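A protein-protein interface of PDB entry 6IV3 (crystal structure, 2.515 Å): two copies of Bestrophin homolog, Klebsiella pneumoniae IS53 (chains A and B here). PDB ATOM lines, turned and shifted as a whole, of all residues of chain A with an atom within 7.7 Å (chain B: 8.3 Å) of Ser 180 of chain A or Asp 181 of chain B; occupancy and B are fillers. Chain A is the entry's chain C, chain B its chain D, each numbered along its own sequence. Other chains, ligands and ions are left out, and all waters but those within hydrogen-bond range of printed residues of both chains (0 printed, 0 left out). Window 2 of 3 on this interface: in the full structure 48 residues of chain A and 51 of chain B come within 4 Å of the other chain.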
ATOM      1  N   ILE A 105       2.354  29.152  19.596  1.00  0.00           N
ATOM      2  CA  ILE A 105       3.458  28.203  19.539  1.00  0.00           C
ATOM      3  C   ILE A 105       3.599  27.619  18.144  1.00  0.00           C
ATOM      4  O   ILE A 105       4.712  27.387  17.667  1.00  0.00           O
ATOM      5  CB  ILE A 105       3.251  27.109  20.604  1.00  0.00           C
ATOM      6  CG1 ILE A 105       3.373  27.716  22.006  1.00  0.00           C
ATOM      7  CG2 ILE A 105       4.238  25.963  20.400  1.00  0.00           C
ATOM      8  CD1 ILE A 105       3.027  26.740  23.165  1.00  0.00           C
ATOM      9  N   LEU A 106       2.467  27.398  17.480  1.00  0.00           N
ATOM     10  CA  LEU A 106       2.406  26.887  16.117  1.00  0.00           C
ATOM     11  C   LEU A 106       1.561  27.842  15.277  1.00  0.00           C
ATOM     12  O   LEU A 106       0.436  27.505  14.877  1.00  0.00           O
ATOM     13  CB  LEU A 106       1.822  25.476  16.097  1.00  0.00           C
ATOM     14  CG  LEU A 106       2.631  24.492  16.937  1.00  0.00           C
ATOM     15  CD1 LEU A 106       1.922  23.142  17.049  1.00  0.00           C
ATOM     16  CD2 LEU A 106       4.038  24.336  16.356  1.00  0.00           C
ATOM     17  N   ILE A 170      -2.638  17.090  19.795  1.00  0.00           N
ATOM     18  CA  ILE A 170      -1.353  17.679  20.194  1.00  0.00           C
ATOM     19  C   ILE A 170      -0.277  16.603  20.313  1.00  0.00           C
ATOM     20  O   ILE A 170       0.922  16.890  20.163  1.00  0.00           O
ATOM     21  CB  ILE A 170      -1.457  18.509  21.494  1.00  0.00           C
ATOM     22  CG1 ILE A 170      -1.932  17.655  22.672  1.00  0.00           C
ATOM     23  CG2 ILE A 170      -2.324  19.735  21.286  1.00  0.00           C
ATOM     24  CD1 ILE A 170      -2.173  18.462  23.976  1.00  0.00           C
ATOM     25  N   LEU A 173       1.197  16.136  16.934  1.00  0.00           N
ATOM     26  CA  LEU A 173       2.090  17.283  16.779  1.00  0.00           C
ATOM     27  C   LEU A 173       3.426  17.054  17.492  1.00  0.00           C
ATOM     28  O   LEU A 173       4.483  17.414  16.964  1.00  0.00           O
ATOM     29  CB  LEU A 173       1.406  18.550  17.295  1.00  0.00           C
ATOM     30  CG  LEU A 173       0.273  19.069  16.413  1.00  0.00           C
ATOM     31  CD1 LEU A 173      -0.484  20.240  17.048  1.00  0.00           C
ATOM     32  CD2 LEU A 173       0.816  19.450  15.019  1.00  0.00           C
ATOM     33  N   ARG A 174       3.402  16.433  18.680  1.00  0.00           N
ATOM     34  CA  ARG A 174       4.646  16.154  19.402  1.00  0.00           C
ATOM     35  C   ARG A 174       5.491  15.095  18.701  1.00  0.00           C
ATOM     36  O   ARG A 174       6.727  15.181  18.725  1.00  0.00           O
ATOM     37  CB  ARG A 174       4.360  15.705  20.840  1.00  0.00           C
ATOM     38  CG  ARG A 174       5.570  15.816  21.767  1.00  0.00           C
ATOM     39  CD  ARG A 174       5.403  14.998  23.066  1.00  0.00           C
ATOM     40  NE  ARG A 174       5.225  13.580  22.775  1.00  0.00           N
ATOM     41  CZ  ARG A 174       6.199  12.679  22.856  1.00  0.00           C
ATOM     42  NH1 ARG A 174       5.966  11.412  22.550  1.00  0.00           N
ATOM     43  NH2 ARG A 174       7.411  13.045  23.253  1.00  0.00           N
ATOM     44  N   GLY A 177       7.747  16.231  15.847  1.00  0.00           N
ATOM     45  CA  GLY A 177       8.733  17.226  16.226  1.00  0.00           C
ATOM     46  C   GLY A 177       8.296  18.673  16.104  1.00  0.00           C
ATOM     47  O   GLY A 177       9.136  19.563  16.243  1.00  0.00           O
ATOM     48  N   LYS A 178       7.013  18.952  15.845  1.00  0.00           N
ATOM     49  CA  LYS A 178       6.575  20.344  15.801  1.00  0.00           C
ATOM     50  C   LYS A 178       6.346  20.923  17.187  1.00  0.00           C
ATOM     51  O   LYS A 178       6.388  22.146  17.364  1.00  0.00           O
ATOM     52  CB  LYS A 178       5.303  20.471  14.981  1.00  0.00           C
ATOM     53  CG  LYS A 178       5.454  19.957  13.579  1.00  0.00           C
ATOM     54  CD  LYS A 178       4.167  20.100  12.813  1.00  0.00           C
ATOM     55  CE  LYS A 178       4.346  19.742  11.349  1.00  0.00           C
ATOM     56  NZ  LYS A 178       2.998  19.614  10.722  1.00  0.00           N
ATOM     57  N   LEU A 179       6.066  20.074  18.166  1.00  0.00           N
ATOM     58  CA  LEU A 179       6.003  20.468  19.559  1.00  0.00           C
ATOM     59  C   LEU A 179       7.159  19.794  20.276  1.00  0.00           C
ATOM     60  O   LEU A 179       7.457  18.620  20.016  1.00  0.00           O
ATOM     61  CB  LEU A 179       4.669  20.064  20.194  1.00  0.00           C
ATOM     62  CG  LEU A 179       3.442  20.930  19.880  1.00  0.00           C
ATOM     63  CD1 LEU A 179       2.138  20.252  20.332  1.00  0.00           C
ATOM     64  CD2 LEU A 179       3.563  22.317  20.497  1.00  0.00           C
ATOM     65  N   SER A 180       7.840  20.543  21.138  1.00  0.00           N
ATOM     66  CA  SER A 180       8.746  19.858  22.038  1.00  0.00           C
ATOM     67  C   SER A 180       7.948  19.225  23.173  1.00  0.00           C
ATOM     68  O   SER A 180       6.750  19.450  23.322  1.00  0.00           O
ATOM     69  CB  SER A 180       9.772  20.822  22.602  1.00  0.00           C
ATOM     70  OG  SER A 180       9.101  21.891  23.235  1.00  0.00           O
ATOM     71  N   ASP A 181       8.639  18.460  24.010  1.00  0.00           N
ATOM     72  CA  ASP A 181       8.018  17.958  25.233  1.00  0.00           C
ATOM     73  C   ASP A 181       7.508  19.089  26.148  1.00  0.00           C
ATOM     74  O   ASP A 181       6.467  18.930  26.792  1.00  0.00           O
ATOM     75  CB  ASP A 181       9.011  17.045  25.953  1.00  0.00           C
ATOM     76  CG  ASP A 181       9.091  15.672  25.315  1.00  0.00           C
ATOM     77  OD1 ASP A 181       8.250  15.388  24.428  1.00  0.00           O
ATOM     78  OD2 ASP A 181       9.974  14.871  25.696  1.00  0.00           O
ATOM     79  N   ILE A 182       8.183  20.244  26.177  1.00  0.00           N
ATOM     80  CA  ILE A 182       7.733  21.354  27.017  1.00  0.00           C
ATOM     81  C   ILE A 182       6.443  21.973  26.469  1.00  0.00           C
ATOM     82  O   ILE A 182       5.485  22.214  27.210  1.00  0.00           O
ATOM     83  CB  ILE A 182       8.822  22.434  27.150  1.00  0.00           C
ATOM     84  CG1 ILE A 182       9.979  21.997  28.045  1.00  0.00           C
ATOM     85  CG2 ILE A 182       8.215  23.721  27.744  1.00  0.00           C
ATOM     86  CD1 ILE A 182      11.119  21.340  27.331  1.00  0.00           C
ATOM     87  N   THR A 183       6.415  22.309  25.181  1.00  0.00           N
ATOM     88  CA  THR A 183       5.240  23.020  24.669  1.00  0.00           C
ATOM     89  C   THR A 183       4.046  22.074  24.570  1.00  0.00           C
ATOM     90  O   THR A 183       2.899  22.457  24.869  1.00  0.00           O
ATOM     91  CB  THR A 183       5.569  23.692  23.324  1.00  0.00           C
ATOM     92  OG1 THR A 183       6.141  22.729  22.428  1.00  0.00           O
ATOM     93  CG2 THR A 183       6.575  24.828  23.523  1.00  0.00           C
ATOM     94  N   TYR A 184       4.315  20.818  24.201  1.00  0.00           N
ATOM     95  CA  TYR A 184       3.334  19.767  24.408  1.00  0.00           C
ATOM     96  C   TYR A 184       2.779  19.829  25.828  1.00  0.00           C
ATOM     97  O   TYR A 184       1.565  19.912  26.024  1.00  0.00           O
ATOM     98  CB  TYR A 184       3.926  18.374  24.149  1.00  0.00           C
ATOM     99  CG  TYR A 184       2.904  17.329  24.520  1.00  0.00           C
ATOM    100  CD1 TYR A 184       1.892  16.999  23.639  1.00  0.00           C
ATOM    101  CD2 TYR A 184       2.889  16.747  25.796  1.00  0.00           C
ATOM    102  CE1 TYR A 184       0.909  16.090  23.988  1.00  0.00           C
ATOM    103  CE2 TYR A 184       1.913  15.846  26.165  1.00  0.00           C
ATOM    104  CZ  TYR A 184       0.920  15.515  25.255  1.00  0.00           C
ATOM    105  OH  TYR A 184      -0.065  14.610  25.599  1.00  0.00           O
ATOM    106  N   GLY A 185       3.671  19.784  26.829  1.00  0.00           N
ATOM    107  CA  GLY A 185       3.241  19.795  28.217  1.00  0.00           C
ATOM    108  C   GLY A 185       2.413  21.014  28.583  1.00  0.00           C
ATOM    109  O   GLY A 185       1.477  20.917  29.396  1.00  0.00           O
ATOM    110  N   LEU A 186       2.737  22.169  27.992  1.00  0.00           N
ATOM    111  CA  LEU A 186       1.979  23.378  28.280  1.00  0.00           C
ATOM    112  C   LEU A 186       0.537  23.205  27.849  1.00  0.00           C
ATOM    113  O   LEU A 186      -0.382  23.663  28.537  1.00  0.00           O
ATOM    114  CB  LEU A 186       2.586  24.588  27.569  1.00  0.00           C
ATOM    115  CG  LEU A 186       3.982  25.082  27.935  1.00  0.00           C
ATOM    116  CD1 LEU A 186       4.278  26.321  27.110  1.00  0.00           C
ATOM    117  CD2 LEU A 186       4.100  25.381  29.429  1.00  0.00           C
ATOM    118  N   GLY B 171       5.552  34.591  21.813  1.00  0.00           N
ATOM    119  CA  GLY B 171       5.790  33.424  20.986  1.00  0.00           C
ATOM    120  C   GLY B 171       6.801  33.704  19.895  1.00  0.00           C
ATOM    121  O   GLY B 171       7.631  32.851  19.573  1.00  0.00           O
ATOM    122  N   LEU B 173       9.174  35.864  20.257  1.00  0.00           N
ATOM    123  CA  LEU B 173      10.434  35.784  20.994  1.00  0.00           C
ATOM    124  C   LEU B 173      10.928  34.345  21.081  1.00  0.00           C
ATOM    125  O   LEU B 173      12.136  34.096  20.997  1.00  0.00           O
ATOM    126  CB  LEU B 173      10.277  36.365  22.395  1.00  0.00           C
ATOM    127  CG  LEU B 173      10.394  37.868  22.535  1.00  0.00           C
ATOM    128  CD1 LEU B 173      10.204  38.253  23.997  1.00  0.00           C
ATOM    129  CD2 LEU B 173      11.743  38.325  22.001  1.00  0.00           C
ATOM    130  N   ARG B 174      10.012  33.381  21.267  1.00  0.00           N
ATOM    131  CA  ARG B 174      10.446  31.989  21.368  1.00  0.00           C
ATOM    132  C   ARG B 174      10.946  31.461  20.024  1.00  0.00           C
ATOM    133  O   ARG B 174      11.973  30.774  19.962  1.00  0.00           O
ATOM    134  CB  ARG B 174       9.317  31.103  21.904  1.00  0.00           C
ATOM    135  CG  ARG B 174       9.810  29.714  22.307  1.00  0.00           C
ATOM    136  CD  ARG B 174       8.712  28.695  22.299  1.00  0.00           C
ATOM    137  NE  ARG B 174       8.080  28.597  20.991  1.00  0.00           N
ATOM    138  CZ  ARG B 174       8.245  27.583  20.155  1.00  0.00           C
ATOM    139  NH1 ARG B 174       7.618  27.583  18.991  1.00  0.00           N
ATOM    140  NH2 ARG B 174       9.017  26.562  20.495  1.00  0.00           N
ATOM    141  N   GLU B 175      10.230  31.763  18.938  1.00  0.00           N
ATOM    142  CA  GLU B 175      10.637  31.272  17.624  1.00  0.00           C
ATOM    143  C   GLU B 175      11.990  31.835  17.211  1.00  0.00           C
ATOM    144  O   GLU B 175      12.801  31.135  16.596  1.00  0.00           O
ATOM    145  CB  GLU B 175       9.579  31.614  16.585  1.00  0.00           C
ATOM    146  CG  GLU B 175       8.874  30.380  16.069  1.00  0.00           C
ATOM    147  CD  GLU B 175       7.509  30.684  15.505  1.00  0.00           C
ATOM    148  OE1 GLU B 175       7.327  31.807  14.979  1.00  0.00           O
ATOM    149  OE2 GLU B 175       6.610  29.813  15.636  1.00  0.00           O
ATOM    150  N   GLY B 177      14.498  32.100  18.921  1.00  0.00           N
ATOM    151  CA  GLY B 177      15.565  31.618  19.765  1.00  0.00           C
ATOM    152  C   GLY B 177      15.888  32.471  20.973  1.00  0.00           C
ATOM    153  O   GLY B 177      16.786  32.107  21.744  1.00  0.00           O
ATOM    154  N   LYS B 178      15.188  33.587  21.182  1.00  0.00           N
ATOM    155  CA  LYS B 178      15.533  34.443  22.312  1.00  0.00           C
ATOM    156  C   LYS B 178      14.995  33.897  23.633  1.00  0.00           C
ATOM    157  O   LYS B 178      15.598  34.128  24.688  1.00  0.00           O
ATOM    158  CB  LYS B 178      15.031  35.865  22.069  1.00  0.00           C
ATOM    159  CG  LYS B 178      15.747  36.564  20.916  1.00  0.00           C
ATOM    160  CD  LYS B 178      15.363  38.026  20.811  1.00  0.00           C
ATOM    161  CE  LYS B 178      15.947  38.671  19.552  1.00  0.00           C
ATOM    162  NZ  LYS B 178      15.257  39.956  19.222  1.00  0.00           N
ATOM    163  N   LEU B 179      13.876  33.182  23.597  1.00  0.00           N
ATOM    164  CA  LEU B 179      13.392  32.420  24.732  1.00  0.00           C
ATOM    165  C   LEU B 179      13.520  30.943  24.404  1.00  0.00           C
ATOM    166  O   LEU B 179      13.298  30.534  23.260  1.00  0.00           O
ATOM    167  CB  LEU B 179      11.933  32.754  25.058  1.00  0.00           C
ATOM    168  CG  LEU B 179      11.551  34.147  25.569  1.00  0.00           C
ATOM    169  CD1 LEU B 179      10.031  34.347  25.474  1.00  0.00           C
ATOM    170  CD2 LEU B 179      12.032  34.415  26.982  1.00  0.00           C
ATOM    171  N   SER B 180      13.901  30.153  25.398  1.00  0.00           N
ATOM    172  CA  SER B 180      13.767  28.712  25.280  1.00  0.00           C
ATOM    173  C   SER B 180      12.318  28.305  25.545  1.00  0.00           C
ATOM    174  O   SER B 180      11.489  29.106  25.990  1.00  0.00           O
ATOM    175  CB  SER B 180      14.702  28.007  26.257  1.00  0.00           C
ATOM    176  OG  SER B 180      14.368  28.327  27.598  1.00  0.00           O
ATOM    177  N   ASP B 181      12.008  27.035  25.279  1.00  0.00           N
ATOM    178  CA  ASP B 181      10.680  26.544  25.630  1.00  0.00           C
ATOM    179  C   ASP B 181      10.403  26.741  27.114  1.00  0.00           C
ATOM    180  O   ASP B 181       9.293  27.128  27.495  1.00  0.00           O
ATOM    181  CB  ASP B 181      10.536  25.083  25.228  1.00  0.00           C
ATOM    182  CG  ASP B 181      10.464  24.908  23.723  1.00  0.00           C
ATOM    183  OD1 ASP B 181      10.190  25.914  23.037  1.00  0.00           O
ATOM    184  OD2 ASP B 181      10.683  23.781  23.219  1.00  0.00           O
ATOM    185  N   ILE B 182      11.416  26.527  27.963  1.00  0.00           N
ATOM    186  CA  ILE B 182      11.247  26.686  29.409  1.00  0.00           C
ATOM    187  C   ILE B 182      10.918  28.137  29.761  1.00  0.00           C
ATOM    188  O   ILE B 182       9.919  28.421  30.439  1.00  0.00           O
ATOM    189  CB  ILE B 182      12.503  26.208  30.159  1.00  0.00           C
ATOM    190  CG1 ILE B 182      12.690  24.699  30.005  1.00  0.00           C
ATOM    191  CG2 ILE B 182      12.407  26.596  31.639  1.00  0.00           C
ATOM    192  CD1 ILE B 182      11.518  23.916  30.508  1.00  0.00           C
ATOM    193  N   THR B 183      11.771  29.081  29.341  1.00  0.00           N
ATOM    194  CA  THR B 183      11.511  30.455  29.765  1.00  0.00           C
ATOM    195  C   THR B 183      10.318  31.047  29.035  1.00  0.00           C
ATOM    196  O   THR B 183       9.693  31.971  29.551  1.00  0.00           O
ATOM    197  CB  THR B 183      12.739  31.368  29.594  1.00  0.00           C
ATOM    198  OG1 THR B 183      13.193  31.359  28.227  1.00  0.00           O
ATOM    199  CG2 THR B 183      13.875  30.930  30.531  1.00  0.00           C
ATOM    200  N   TYR B 184       9.975  30.532  27.855  1.00  0.00           N
ATOM    201  CA  TYR B 184       8.673  30.863  27.293  1.00  0.00           C
ATOM    202  C   TYR B 184       7.549  30.389  28.221  1.00  0.00           C
ATOM    203  O   TYR B 184       6.606  31.139  28.501  1.00  0.00           O
ATOM    204  CB  TYR B 184       8.531  30.256  25.891  1.00  0.00           C
ATOM    205  CG  TYR B 184       7.119  30.313  25.369  1.00  0.00           C
ATOM    206  CD1 TYR B 184       6.665  31.416  24.652  1.00  0.00           C
ATOM    207  CD2 TYR B 184       6.222  29.265  25.612  1.00  0.00           C
ATOM    208  CE1 TYR B 184       5.346  31.466  24.186  1.00  0.00           C
ATOM    209  CE2 TYR B 184       4.930  29.304  25.151  1.00  0.00           C
ATOM    210  CZ  TYR B 184       4.492  30.407  24.448  1.00  0.00           C
ATOM    211  OH  TYR B 184       3.197  30.429  24.005  1.00  0.00           O
ATOM    212  N   GLY B 185       7.648  29.151  28.729  1.00  0.00           N
ATOM    213  CA  GLY B 185       6.591  28.606  29.564  1.00  0.00           C
ATOM    214  C   GLY B 185       6.398  29.372  30.858  1.00  0.00           C
ATOM    215  O   GLY B 185       5.264  29.498  31.354  1.00  0.00           O
ATOM    216  N   LEU B 186       7.494  29.907  31.420  1.00  0.00           N
ATOM    217  CA  LEU B 186       7.356  30.652  32.668  1.00  0.00           C
ATOM    218  C   LEU B 186       6.601  31.956  32.476  1.00  0.00           C
ATOM    219  O   LEU B 186       6.115  32.536  33.453  1.00  0.00           O
ATOM    220  CB  LEU B 186       8.704  30.965  33.294  1.00  0.00           C
ATOM    221  CG  LEU B 186       9.648  29.827  33.651  1.00  0.00           C
ATOM    222  CD1 LEU B 186      11.127  30.263  33.561  1.00  0.00           C
ATOM    223  CD2 LEU B 186       9.286  29.406  35.045  1.00  0.00           C
ATOM    224  N   MET B 187       6.526  32.460  31.238  1.00  0.00           N
ATOM    225  CA  MET B 187       5.744  33.657  30.962  1.00  0.00           C
ATOM    226  C   MET B 187       4.347  33.290  30.512  1.00  0.00           C
ATOM    227  O   MET B 187       3.377  33.996  30.836  1.00  0.00           O
ATOM    228  CB  MET B 187       6.480  34.506  29.922  1.00  0.00           C
ATOM    229  CG  MET B 187       7.930  34.816  30.355  1.00  0.00           C
ATOM    230  SD  MET B 187       9.016  35.758  29.224  1.00  0.00           S
ATOM    231  CE  MET B 187       8.011  37.193  29.012  1.00  0.00           C
ATOM    232  N   ASP B 188       4.233  32.152  29.813  1.00  0.00           N
ATOM    233  CA  ASP B 188       2.926  31.618  29.459  1.00  0.00           C
ATOM    234  C   ASP B 188       2.045  31.472  30.696  1.00  0.00           C
ATOM    235  O   ASP B 188       0.856  31.835  30.672  1.00  0.00           O
ATOM    236  CB  ASP B 188       3.091  30.275  28.739  1.00  0.00           C
ATOM    237  CG  ASP B 188       1.847  29.881  27.944  1.00  0.00           C
ATOM    238  OD1 ASP B 188       1.732  30.287  26.770  1.00  0.00           O
ATOM    239  OD2 ASP B 188       0.975  29.184  28.500  1.00  0.00           O
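Among the printed residues, pairs that only touch across the chains: Ile 105 of chain A with Glu 175 of chain B (3.7 Å), Ile 105 of chain A with Tyr 184 of chain B (3.4 Å), Ile 182 of chain A with Asp 181 of chain B (3.6 Å), Ile 182 of chain A with Ile 182 of chain B (3.5 Å), Thr 183 of chain A with Asp 181 of chain B (3.8 Å) and Leu 186 of chain A with Tyr 184 of chain B (3.6 Å).
The side-chain hydroxyl (OG) of Ser 180 of chain A sits at hydrogen-bond distance from the side-chain carboxylate (OD2) of Asp 181 of chain B, 2.5 Å away.
The guanidinium group of Arg 174 of chain B is in hydrogen-bond range of the backbone carbonyl oxygen of Ile 105 of chain A, at 3.2 Å.
Of the 16 printed residues of chain B, 5 touch a printed residue of chain A.
Printed residues of chain B that touch a printed residue of chain A: Arg 174, Glu 175, Asp 181, Ile 182 and Tyr 184.
Of the 15 printed residues of chain A, 5 touch a printed residue of chain B.
Hydrophobic or aromatic side chains of chain A within 4 Å of the printed part of chain B: Ile 105, Ile 182 and Leu 186.
Along chain A the printed residues that touch a printed residue of chain B span positions 105 to 186.
The side-chain hydroxyl (OG) of Ser 180 of chain B sits close to the backbone NH (N) of Ile 182 of chain B (3.5 Å).
The side-chain carboxylate of Asp 181 of chain B lies within salt-bridge range of the guanidinium group of Arg 174 of chain B (2.9 Å).
The backbone NH of Ser 180 of chain A lies within hydrogen-bond range of the side-chain hydroxyl of Thr 183 of chain A (3.1 Å).
OH of Tyr 184 of chain B lies within hydrogen-bond range of OD1 of Asp 188 of chain B, 3.1 Å away.
N of Ile 182 of chain A sits close to OG of Ser 180 of chain A (3.5 Å).
Ile 182 of chain A touches Asp 181 of chain B, but with the chains exchanged Asp 181 of chain A does not touch Ile 182 of chain B (7.6 Å).
Ile 182 of chain A touches its own counterpart, Ile 182 of chain B.
Thr 183 of chain A touches Asp 181 of chain B, but with the chains exchanged Asp 181 of chain A does not touch Thr 183 of chain B (11.3 Å).
Leu 186 of chain A touches Tyr 184 of chain B, but with the chains exchanged Tyr 184 of chain A does not touch Leu 186 of chain B (12.0 Å).
12 positions are printed for both chains.
Of the printed residues of chain B, Ile 105 of chain A touches Arg 174 (3.2 Å), Glu 175 (3.7 Å) and Tyr 184 (3.4 Å).
Gly 177 of chain A touches none of the printed residues of chain B.
Ser 180 of chain A touches just one residue of chain B: Asp 181 (2.5 Å).
Of the printed residues of chain B, Thr 183 of chain A touches Asp 181.
Printed residues of chain B within 4 Å of Leu 186 of chain A: Tyr 184.
No residue of chain A comes within 4 Å of Ser 180 of chain B.
Asp 181 of chain B touches three residues of chain A.
Of the printed residues of chain A, Ile 182 of chain B touches Ile 182 (3.5 Å).
The nearest residue of chain B that does not touch Ser 180 of chain A is Arg 174 of chain B (5.4 Å).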
